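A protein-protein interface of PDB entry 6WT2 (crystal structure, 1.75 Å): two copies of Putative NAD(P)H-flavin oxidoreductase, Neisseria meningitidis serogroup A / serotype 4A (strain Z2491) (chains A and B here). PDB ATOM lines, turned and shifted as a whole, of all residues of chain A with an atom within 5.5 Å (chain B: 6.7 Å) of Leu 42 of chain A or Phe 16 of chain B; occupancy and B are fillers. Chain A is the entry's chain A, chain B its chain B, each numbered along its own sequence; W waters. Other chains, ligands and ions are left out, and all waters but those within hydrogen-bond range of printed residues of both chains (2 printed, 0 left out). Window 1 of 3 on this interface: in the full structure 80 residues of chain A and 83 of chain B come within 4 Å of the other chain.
No position is printed for both chains.
The side-chain amide oxygen (OD1) of Asn 155 of chain A is in hydrogen-bond range of the side-chain hydroxyl (OG1) of Thr 158 of chain B (2.7 Å).
Among the printed residues, merely in contact across the chains: Asn 155 of chain A with Gly 154 of chain B, Asn 155 of chain A with Phe 16 of chain B, Phe 38 of chain A with Val 12 of chain B, Leu 42 of chain A with Phe 16 of chain B, Leu 45 of chain A with Phe 16 of chain B, Leu 45 of chain A with Arg 19 of chain B, Leu 45 of chain A with Lys 17 of chain B and Phe 38 of chain A with Leu 13 of chain B.
O of Gly 154 of chain B sits at hydrogen-bond distance from OG1 of Thr 158 of chain B. The side-chain hydroxyl of Ser 46 of chain A is in hydrogen-bond range of the side-chain amide nitrogen of Asn 155 of chain A (2.9 Å). OG of Ser 46 of chain A lies within hydrogen-bond range of O of Leu 42 of chain A.
Of the 14 printed residues of chain B, 7 touch a printed residue of chain A. Hydrophobic or aromatic side chains of chain B that line the printed part of chain A: Val 12, Leu 13 and Phe 16. Printed residues of chain A that touch a printed residue of chain B: Phe 38, Leu 42, Leu 45 and Asn 155. Among the printed residues, no Asp or Glu carboxylate lies within 4 Å of a Lys or Arg side-chain nitrogen of the other chain.
Printed residues of chain B within 4 Å of Phe 38 of chain A: Val 12 and Leu 13. Leu 40 of chain A touches none of the printed residues of chain B. Glu 41 of chain A touches none of the printed residues of chain B. Leu 42 of chain A touches just one residue of chain B: Phe 16 (3.6 Å). Of the printed residues of chain A, Lys 17 of chain B touches Leu 45. Of the printed residues of chain A, Arg 19 of chain B touches Leu 45. Printed residues of chain A within 4 Å of Gly 154 of chain B: Asn 155 (3.6 Å). The nearest residue of chain B that does not touch Leu 42 of chain A is Leu 13 of chain B (4.1 Å). The nearest residue of chain A that does not touch Phe 16 of chain B is Ser 46 of chain A (4.5 Å). The nearest printed residue of chain B that does not touch Asn 155 of chain A is Arg 19 of chain B (5.8 Å).
Water W1 bridges NH2 of Arg 19 of chain B (2.8 Å) and O of Leu 45 of chain A (2.8 Å). Water W2 lies within hydrogen-bond range of ND2 of Asn 155 of chain A (2.9 Å), OG1 of Thr 158 of chain B (3.0 Å) and O of Gly 154 of chain B (3.2 Å).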
ATOM      1  N   GLN A  37     -11.889 -17.375 -20.388  1.00  0.00           N
ATOM      2  CA  GLN A  37     -11.323 -16.792 -19.175  1.00  0.00           C
ATOM      3  C   GLN A  37      -9.853 -17.155 -19.040  1.00  0.00           C
ATOM      4  O   GLN A  37      -9.046 -16.354 -18.553  1.00  0.00           O
ATOM      5  CB  GLN A  37     -12.083 -17.263 -17.936  1.00  0.00           C
ATOM      6  CG  GLN A  37     -13.524 -16.800 -17.852  1.00  0.00           C
ATOM      7  CD  GLN A  37     -13.663 -15.354 -17.396  1.00  0.00           C
ATOM      8  OE1 GLN A  37     -12.983 -14.916 -16.464  1.00  0.00           O
ATOM      9  NE2 GLN A  37     -14.552 -14.606 -18.053  1.00  0.00           N
ATOM     10  N   PHE A  38      -9.501 -18.390 -19.408  1.00  0.00           N
ATOM     11  CA  PHE A  38      -8.102 -18.809 -19.404  1.00  0.00           C
ATOM     12  C   PHE A  38      -7.265 -17.942 -20.341  1.00  0.00           C
ATOM     13  O   PHE A  38      -6.148 -17.538 -19.996  1.00  0.00           O
ATOM     14  CB  PHE A  38      -8.017 -20.294 -19.774  1.00  0.00           C
ATOM     15  CG  PHE A  38      -6.742 -20.695 -20.488  1.00  0.00           C
ATOM     16  CD1 PHE A  38      -5.564 -20.898 -19.782  1.00  0.00           C
ATOM     17  CD2 PHE A  38      -6.740 -20.904 -21.865  1.00  0.00           C
ATOM     18  CE1 PHE A  38      -4.403 -21.279 -20.442  1.00  0.00           C
ATOM     19  CE2 PHE A  38      -5.581 -21.286 -22.532  1.00  0.00           C
ATOM     20  CZ  PHE A  38      -4.413 -21.470 -21.822  1.00  0.00           C
ATOM     21  N   ILE A  39      -7.805 -17.615 -21.517  1.00  0.00           N
ATOM     22  CA  ILE A  39      -7.085 -16.759 -22.461  1.00  0.00           C
ATOM     23  C   ILE A  39      -6.891 -15.362 -21.874  1.00  0.00           C
ATOM     24  O   ILE A  39      -5.789 -14.800 -21.908  1.00  0.00           O
ATOM     25  CB  ILE A  39      -7.829 -16.714 -23.808  1.00  0.00           C
ATOM     26  CG1 ILE A  39      -7.835 -18.101 -24.458  1.00  0.00           C
ATOM     27  CG2 ILE A  39      -7.198 -15.694 -24.742  1.00  0.00           C
ATOM     28  CD1 ILE A  39      -8.719 -18.168 -25.709  1.00  0.00           C
ATOM     29  N   LEU A  40      -7.958 -14.774 -21.326  1.00  0.00           N
ATOM     30  CA  LEU A  40      -7.807 -13.461 -20.695  1.00  0.00           C
ATOM     31  C   LEU A  40      -6.773 -13.506 -19.578  1.00  0.00           C
ATOM     32  O   LEU A  40      -6.039 -12.532 -19.351  1.00  0.00           O
ATOM     33  CB  LEU A  40      -9.149 -12.966 -20.151  1.00  0.00           C
ATOM     34  CG  LEU A  40     -10.266 -12.682 -21.162  1.00  0.00           C
ATOM     35  CD1 LEU A  40     -11.601 -12.491 -20.426  1.00  0.00           C
ATOM     36  CD2 LEU A  40      -9.954 -11.450 -22.002  1.00  0.00           C
ATOM     37  N   GLU A  41      -6.702 -14.628 -18.864  1.00  0.00           N
ATOM     38  CA  GLU A  41      -5.768 -14.715 -17.746  1.00  0.00           C
ATOM     39  C   GLU A  41      -4.328 -14.670 -18.234  1.00  0.00           C
ATOM     40  O   GLU A  41      -3.461 -14.084 -17.570  1.00  0.00           O
ATOM     41  CB  GLU A  41      -6.028 -15.980 -16.932  1.00  0.00           C
ATOM     42  CG  GLU A  41      -5.298 -15.998 -15.598  1.00  0.00           C
ATOM     43  CD  GLU A  41      -5.832 -14.953 -14.617  1.00  0.00           C
ATOM     44  OE1 GLU A  41      -7.047 -14.636 -14.673  1.00  0.00           O
ATOM     45  OE2 GLU A  41      -5.031 -14.452 -13.792  1.00  0.00           O
ATOM     46  N   LEU A  42      -4.051 -15.262 -19.399  1.00  0.00           N
ATOM     47  CA  LEU A  42      -2.700 -15.185 -19.937  1.00  0.00           C
ATOM     48  C   LEU A  42      -2.298 -13.740 -20.186  1.00  0.00           C
ATOM     49  O   LEU A  42      -1.144 -13.361 -19.960  1.00  0.00           O
ATOM     50  CB  LEU A  42      -2.592 -16.004 -21.224  1.00  0.00           C
ATOM     51  CG  LEU A  42      -2.939 -17.483 -21.078  1.00  0.00           C
ATOM     52  CD1 LEU A  42      -3.116 -18.121 -22.449  1.00  0.00           C
ATOM     53  CD2 LEU A  42      -1.860 -18.202 -20.291  1.00  0.00           C
ATOM     54  N   GLY A  43      -3.242 -12.912 -20.633  1.00  0.00           N
ATOM     55  CA  GLY A  43      -2.933 -11.505 -20.815  1.00  0.00           C
ATOM     56  C   GLY A  43      -2.791 -10.767 -19.497  1.00  0.00           C
ATOM     57  O   GLY A  43      -1.880  -9.952 -19.331  1.00  0.00           O
ATOM     58  N   ARG A  44      -3.691 -11.037 -18.547  1.00  0.00           N
ATOM     59  CA  ARG A  44      -3.596 -10.437 -17.215  1.00  0.00           C
ATOM     60  C   ARG A  44      -2.231 -10.686 -16.583  1.00  0.00           C
ATOM     61  O   ARG A  44      -1.619  -9.777 -16.009  1.00  0.00           O
ATOM     62  CB  ARG A  44      -4.698 -10.993 -16.311  1.00  0.00           C
ATOM     63  CG  ARG A  44      -4.479 -10.710 -14.835  1.00  0.00           C
ATOM     64  CD  ARG A  44      -5.742 -10.934 -14.011  1.00  0.00           C
ATOM     65  NE  ARG A  44      -5.512 -10.510 -12.628  1.00  0.00           N
ATOM     66  CZ  ARG A  44      -5.093 -11.307 -11.652  1.00  0.00           C
ATOM     67  NH1 ARG A  44      -4.886 -12.596 -11.882  1.00  0.00           N
ATOM     68  NH2 ARG A  44      -4.883 -10.812 -10.440  1.00  0.00           N
ATOM     69  N   LEU A  45      -1.750 -11.920 -16.657  1.00  0.00           N
ATOM     70  CA  LEU A  45      -0.514 -12.293 -15.990  1.00  0.00           C
ATOM     71  C   LEU A  45       0.742 -11.909 -16.771  1.00  0.00           C
ATOM     72  O   LEU A  45       1.856 -12.149 -16.277  1.00  0.00           O
ATOM     73  CB  LEU A  45      -0.519 -13.793 -15.715  1.00  0.00           C
ATOM     74  CG  LEU A  45      -1.627 -14.337 -14.823  1.00  0.00           C
ATOM     75  CD1 LEU A  45      -1.561 -15.854 -14.789  1.00  0.00           C
ATOM     76  CD2 LEU A  45      -1.548 -13.745 -13.397  1.00  0.00           C
ATOM     77  N   SER A  46       0.603 -11.311 -17.952  1.00  0.00           N
ATOM     78  CA  SER A  46       1.773 -10.985 -18.744  1.00  0.00           C
ATOM     79  C   SER A  46       2.609  -9.944 -18.006  1.00  0.00           C
ATOM     80  O   SER A  46       2.078  -9.180 -17.196  1.00  0.00           O
ATOM     81  CB  SER A  46       1.378 -10.459 -20.124  1.00  0.00           C
ATOM     82  OG  SER A  46       0.836 -11.500 -20.924  1.00  0.00           O
ATOM     83  N   ALA A 152       1.228  -9.067 -23.995  1.00  0.00           N
ATOM     84  CA  ALA A 152      -0.024  -9.734 -23.655  1.00  0.00           C
ATOM     85  C   ALA A 152      -0.646 -10.383 -24.877  1.00  0.00           C
ATOM     86  O   ALA A 152      -1.139 -11.513 -24.805  1.00  0.00           O
ATOM     87  CB  ALA A 152      -1.000  -8.738 -23.037  1.00  0.00           C
ATOM     88  N   ASN A 155       1.253 -13.621 -25.677  1.00  0.00           N
ATOM     89  CA  ASN A 155       1.004 -14.673 -24.692  1.00  0.00           C
ATOM     90  C   ASN A 155      -0.393 -15.267 -24.832  1.00  0.00           C
ATOM     91  O   ASN A 155      -0.565 -16.488 -24.755  1.00  0.00           O
ATOM     92  CB  ASN A 155       1.204 -14.126 -23.284  1.00  0.00           C
ATOM     93  CG  ASN A 155       2.660 -14.046 -22.892  1.00  0.00           C
ATOM     94  OD1 ASN A 155       3.508 -14.785 -23.421  1.00  0.00           O
ATOM     95  ND2 ASN A 155       2.964 -13.176 -21.933  1.00  0.00           N
ATOM     96  N   MET A 156      -1.402 -14.428 -25.026  1.00  0.00           N
ATOM     97  CA  MET A 156      -2.756 -14.931 -25.211  1.00  0.00           C
ATOM     98  C   MET A 156      -2.870 -15.841 -26.443  1.00  0.00           C
ATOM     99  O   MET A 156      -3.470 -16.921 -26.373  1.00  0.00           O
ATOM    100  CB  MET A 156      -3.729 -13.759 -25.300  1.00  0.00           C
ATOM    101  CG  MET A 156      -3.887 -13.068 -23.960  1.00  0.00           C
ATOM    102  SD  MET A 156      -4.730 -11.336 -24.121  1.00  0.00           S
ATOM    103  CE  MET A 156      -6.419 -11.960 -24.836  1.00  0.00           C
ATOM    104  N   GLY A 159      -0.751 -19.185 -25.811  1.00  0.00           N
ATOM    105  CA  GLY A 159      -1.435 -20.034 -24.854  1.00  0.00           C
ATOM    106  C   GLY A 159      -2.710 -20.625 -25.421  1.00  0.00           C
ATOM    107  O   GLY A 159      -2.983 -21.812 -25.249  1.00  0.00           O
ATOM    108  N   ALA A 160      -3.518 -19.795 -26.089  1.00  0.00           N
ATOM    109  CA  ALA A 160      -4.699 -20.306 -26.788  1.00  0.00           C
ATOM    110  C   ALA A 160      -4.345 -21.455 -27.722  1.00  0.00           C
ATOM    111  O   ALA A 160      -4.971 -22.524 -27.690  1.00  0.00           O
ATOM    112  CB  ALA A 160      -5.359 -19.188 -27.591  1.00  0.00           C
ATOM    113  N   GLN B  11      -2.776 -27.425 -17.596  1.00  0.00           N
ATOM    114  CA  GLN B  11      -1.335 -27.634 -17.683  1.00  0.00           C
ATOM    115  C   GLN B  11      -0.655 -26.440 -18.338  1.00  0.00           C
ATOM    116  O   GLN B  11       0.456 -26.059 -17.954  1.00  0.00           O
ATOM    117  CB  GLN B  11      -1.023 -28.918 -18.458  1.00  0.00           C
ATOM    118  CG  GLN B  11       0.341 -29.526 -18.103  1.00  0.00           C
ATOM    119  CD  GLN B  11       0.799 -30.638 -19.050  1.00  0.00           C
ATOM    120  OE1 GLN B  11       0.558 -30.591 -20.262  1.00  0.00           O
ATOM    121  NE2 GLN B  11       1.472 -31.642 -18.493  1.00  0.00           N
ATOM    122  N   VAL B  12      -1.305 -25.835 -19.331  1.00  0.00           N
ATOM    123  CA  VAL B  12      -0.722 -24.672 -19.984  1.00  0.00           C
ATOM    124  C   VAL B  12      -0.596 -23.525 -18.995  1.00  0.00           C
ATOM    125  O   VAL B  12       0.461 -22.890 -18.879  1.00  0.00           O
ATOM    126  CB  VAL B  12      -1.555 -24.261 -21.208  1.00  0.00           C
ATOM    127  CG1 VAL B  12      -1.091 -22.916 -21.715  1.00  0.00           C
ATOM    128  CG2 VAL B  12      -1.415 -25.311 -22.317  1.00  0.00           C
ATOM    129  N   LEU B  13      -1.682 -23.237 -18.279  1.00  0.00           N
ATOM    130  CA  LEU B  13      -1.670 -22.148 -17.313  1.00  0.00           C
ATOM    131  C   LEU B  13      -0.666 -22.414 -16.203  1.00  0.00           C
ATOM    132  O   LEU B  13       0.032 -21.495 -15.754  1.00  0.00           O
ATOM    133  CB  LEU B  13      -3.081 -21.944 -16.748  1.00  0.00           C
ATOM    134  CG  LEU B  13      -3.295 -20.759 -15.802  1.00  0.00           C
ATOM    135  CD1 LEU B  13      -2.885 -19.447 -16.473  1.00  0.00           C
ATOM    136  CD2 LEU B  13      -4.740 -20.687 -15.321  1.00  0.00           C
ATOM    137  N   SER B  14      -0.566 -23.669 -15.757  1.00  0.00           N
ATOM    138  CA  SER B  14       0.346 -23.996 -14.665  1.00  0.00           C
ATOM    139  C   SER B  14       1.788 -23.707 -15.056  1.00  0.00           C
ATOM    140  O   SER B  14       2.548 -23.111 -14.284  1.00  0.00           O
ATOM    141  CB  SER B  14       0.192 -25.463 -14.267  1.00  0.00           C
ATOM    142  OG  SER B  14      -0.977 -25.658 -13.500  1.00  0.00           O
ATOM    143  N   ALA B  15       2.182 -24.137 -16.258  1.00  0.00           N
ATOM    144  CA  ALA B  15       3.549 -23.922 -16.712  1.00  0.00           C
ATOM    145  C   ALA B  15       3.801 -22.451 -17.011  1.00  0.00           C
ATOM    146  O   ALA B  15       4.903 -21.944 -16.760  1.00  0.00           O
ATOM    147  CB  ALA B  15       3.834 -24.780 -17.942  1.00  0.00           C
ATOM    148  N   PHE B  16       2.792 -21.754 -17.551  1.00  0.00           N
ATOM    149  CA  PHE B  16       2.915 -20.324 -17.825  1.00  0.00           C
ATOM    150  C   PHE B  16       3.282 -19.538 -16.567  1.00  0.00           C
ATOM    151  O   PHE B  16       4.077 -18.587 -16.624  1.00  0.00           O
ATOM    152  CB  PHE B  16       1.603 -19.811 -18.422  1.00  0.00           C
ATOM    153  CG  PHE B  16       1.628 -18.360 -18.827  1.00  0.00           C
ATOM    154  CD1 PHE B  16       1.926 -18.002 -20.137  1.00  0.00           C
ATOM    155  CD2 PHE B  16       1.311 -17.357 -17.909  1.00  0.00           C
ATOM    156  CE1 PHE B  16       1.934 -16.674 -20.528  1.00  0.00           C
ATOM    157  CE2 PHE B  16       1.317 -16.023 -18.286  1.00  0.00           C
ATOM    158  CZ  PHE B  16       1.628 -15.679 -19.599  1.00  0.00           C
ATOM    159  N   LYS B  17       2.706 -19.913 -15.421  1.00  0.00           N
ATOM    160  CA  LYS B  17       2.995 -19.261 -14.150  1.00  0.00           C
ATOM    161  C   LYS B  17       4.411 -19.523 -13.659  1.00  0.00           C
ATOM    162  O   LYS B  17       4.800 -18.961 -12.628  1.00  0.00           O
ATOM    163  CB  LYS B  17       1.996 -19.713 -13.087  1.00  0.00           C
ATOM    164  CG  LYS B  17       0.562 -19.311 -13.367  1.00  0.00           C
ATOM    165  CD  LYS B  17      -0.353 -19.902 -12.313  1.00  0.00           C
ATOM    166  CE  LYS B  17      -1.813 -19.799 -12.711  1.00  0.00           C
ATOM    167  NZ  LYS B  17      -2.496 -18.632 -12.108  1.00  0.00           N
ATOM    168  N   ASN B  18       5.187 -20.363 -14.355  1.00  0.00           N
ATOM    169  CA  ASN B  18       6.602 -20.479 -14.023  1.00  0.00           C
ATOM    170  C   ASN B  18       7.319 -19.152 -14.215  1.00  0.00           C
ATOM    171  O   ASN B  18       8.321 -18.888 -13.542  1.00  0.00           O
ATOM    172  CB  ASN B  18       7.286 -21.552 -14.883  1.00  0.00           C
ATOM    173  CG  ASN B  18       6.815 -22.967 -14.572  1.00  0.00           C
ATOM    174  OD1 ASN B  18       6.213 -23.228 -13.538  1.00  0.00           O
ATOM    175  ND2 ASN B  18       7.112 -23.892 -15.473  1.00  0.00           N
ATOM    176  N   ARG B  19       6.832 -18.308 -15.126  1.00  0.00           N
ATOM    177  CA  ARG B  19       7.599 -17.136 -15.533  1.00  0.00           C
ATOM    178  C   ARG B  19       7.467 -16.038 -14.497  1.00  0.00           C
ATOM    179  O   ARG B  19       6.373 -15.511 -14.284  1.00  0.00           O
ATOM    180  CB  ARG B  19       7.161 -16.596 -16.888  1.00  0.00           C
ATOM    181  CG  ARG B  19       8.244 -15.682 -17.494  1.00  0.00           C
ATOM    182  CD  ARG B  19       7.667 -14.501 -18.275  1.00  0.00           C
ATOM    183  NE  ARG B  19       6.616 -13.842 -17.486  1.00  0.00           N
ATOM    184  CZ  ARG B  19       6.822 -12.881 -16.580  1.00  0.00           C
ATOM    185  NH1 ARG B  19       8.047 -12.423 -16.353  1.00  0.00           N
ATOM    186  NH2 ARG B  19       5.794 -12.373 -15.896  1.00  0.00           N
ATOM    187  N   LYS B  20       8.592 -15.678 -13.886  1.00  0.00           N
ATOM    188  CA  LYS B  20       8.693 -14.535 -12.993  1.00  0.00           C
ATOM    189  C   LYS B  20       9.963 -13.787 -13.348  1.00  0.00           C
ATOM    190  O   LYS B  20      10.966 -14.412 -13.693  1.00  0.00           O
ATOM    191  CB  LYS B  20       8.722 -14.976 -11.532  1.00  0.00           C
ATOM    192  CG  LYS B  20       7.520 -15.831 -11.127  1.00  0.00           C
ATOM    193  CD  LYS B  20       7.681 -16.329  -9.715  1.00  0.00           C
ATOM    194  CE  LYS B  20       6.835 -17.556  -9.435  1.00  0.00           C
ATOM    195  NZ  LYS B  20       6.959 -17.926  -7.994  1.00  0.00           N
ATOM    196  N   GLY B 154       8.006 -11.738 -25.605  1.00  0.00           N
ATOM    197  CA  GLY B 154       7.047 -12.439 -24.761  1.00  0.00           C
ATOM    198  C   GLY B 154       7.074 -13.945 -24.969  1.00  0.00           C
ATOM    199  O   GLY B 154       7.065 -14.713 -24.005  1.00  0.00           O
ATOM    200  N   THR B 158       8.172 -16.718 -22.142  1.00  0.00           N
ATOM    201  CA  THR B 158       7.147 -17.670 -21.724  1.00  0.00           C
ATOM    202  C   THR B 158       7.579 -19.105 -22.009  1.00  0.00           C
ATOM    203  O   THR B 158       7.500 -19.977 -21.133  1.00  0.00           O
ATOM    204  CB  THR B 158       5.825 -17.347 -22.422  1.00  0.00           C
ATOM    205  OG1 THR B 158       5.299 -16.135 -21.865  1.00  0.00           O
ATOM    206  CG2 THR B 158       4.815 -18.485 -22.235  1.00  0.00           C
ATOM    207  N   ALA B 161      10.307 -20.259 -19.686  1.00  0.00           N
ATOM    208  CA  ALA B 161       9.857 -20.521 -18.326  1.00  0.00           C
ATOM    209  C   ALA B 161       9.104 -21.842 -18.233  1.00  0.00           C
ATOM    210  O   ALA B 161       9.265 -22.586 -17.257  1.00  0.00           O
ATOM    211  CB  ALA B 161       8.985 -19.366 -17.844  1.00  0.00           C
ATOM    212  N   MET B 162       8.289 -22.149 -19.238  1.00  0.00           N
ATOM    213  CA  MET B 162       7.528 -23.391 -19.271  1.00  0.00           C
ATOM    214  C   MET B 162       8.465 -24.589 -19.241  1.00  0.00           C
ATOM    215  O   MET B 162       8.123 -25.644 -18.704  1.00  0.00           O
ATOM    216  CB  MET B 162       6.636 -23.444 -20.520  1.00  0.00           C
ATOM    217  CG  MET B 162       5.508 -22.420 -20.500  1.00  0.00           C
ATOM    218  SD  MET B 162       4.323 -22.666 -22.027  1.00  0.00           S
ATOM    219  CE  MET B 162       3.320 -24.179 -21.353  1.00  0.00           C
HETATM  220  O   HOH W   1       3.813 -14.023 -16.907  1.00  0.00           O
HETATM  221  O   HOH W   2       5.845 -13.225 -21.474  1.00  0.00           O
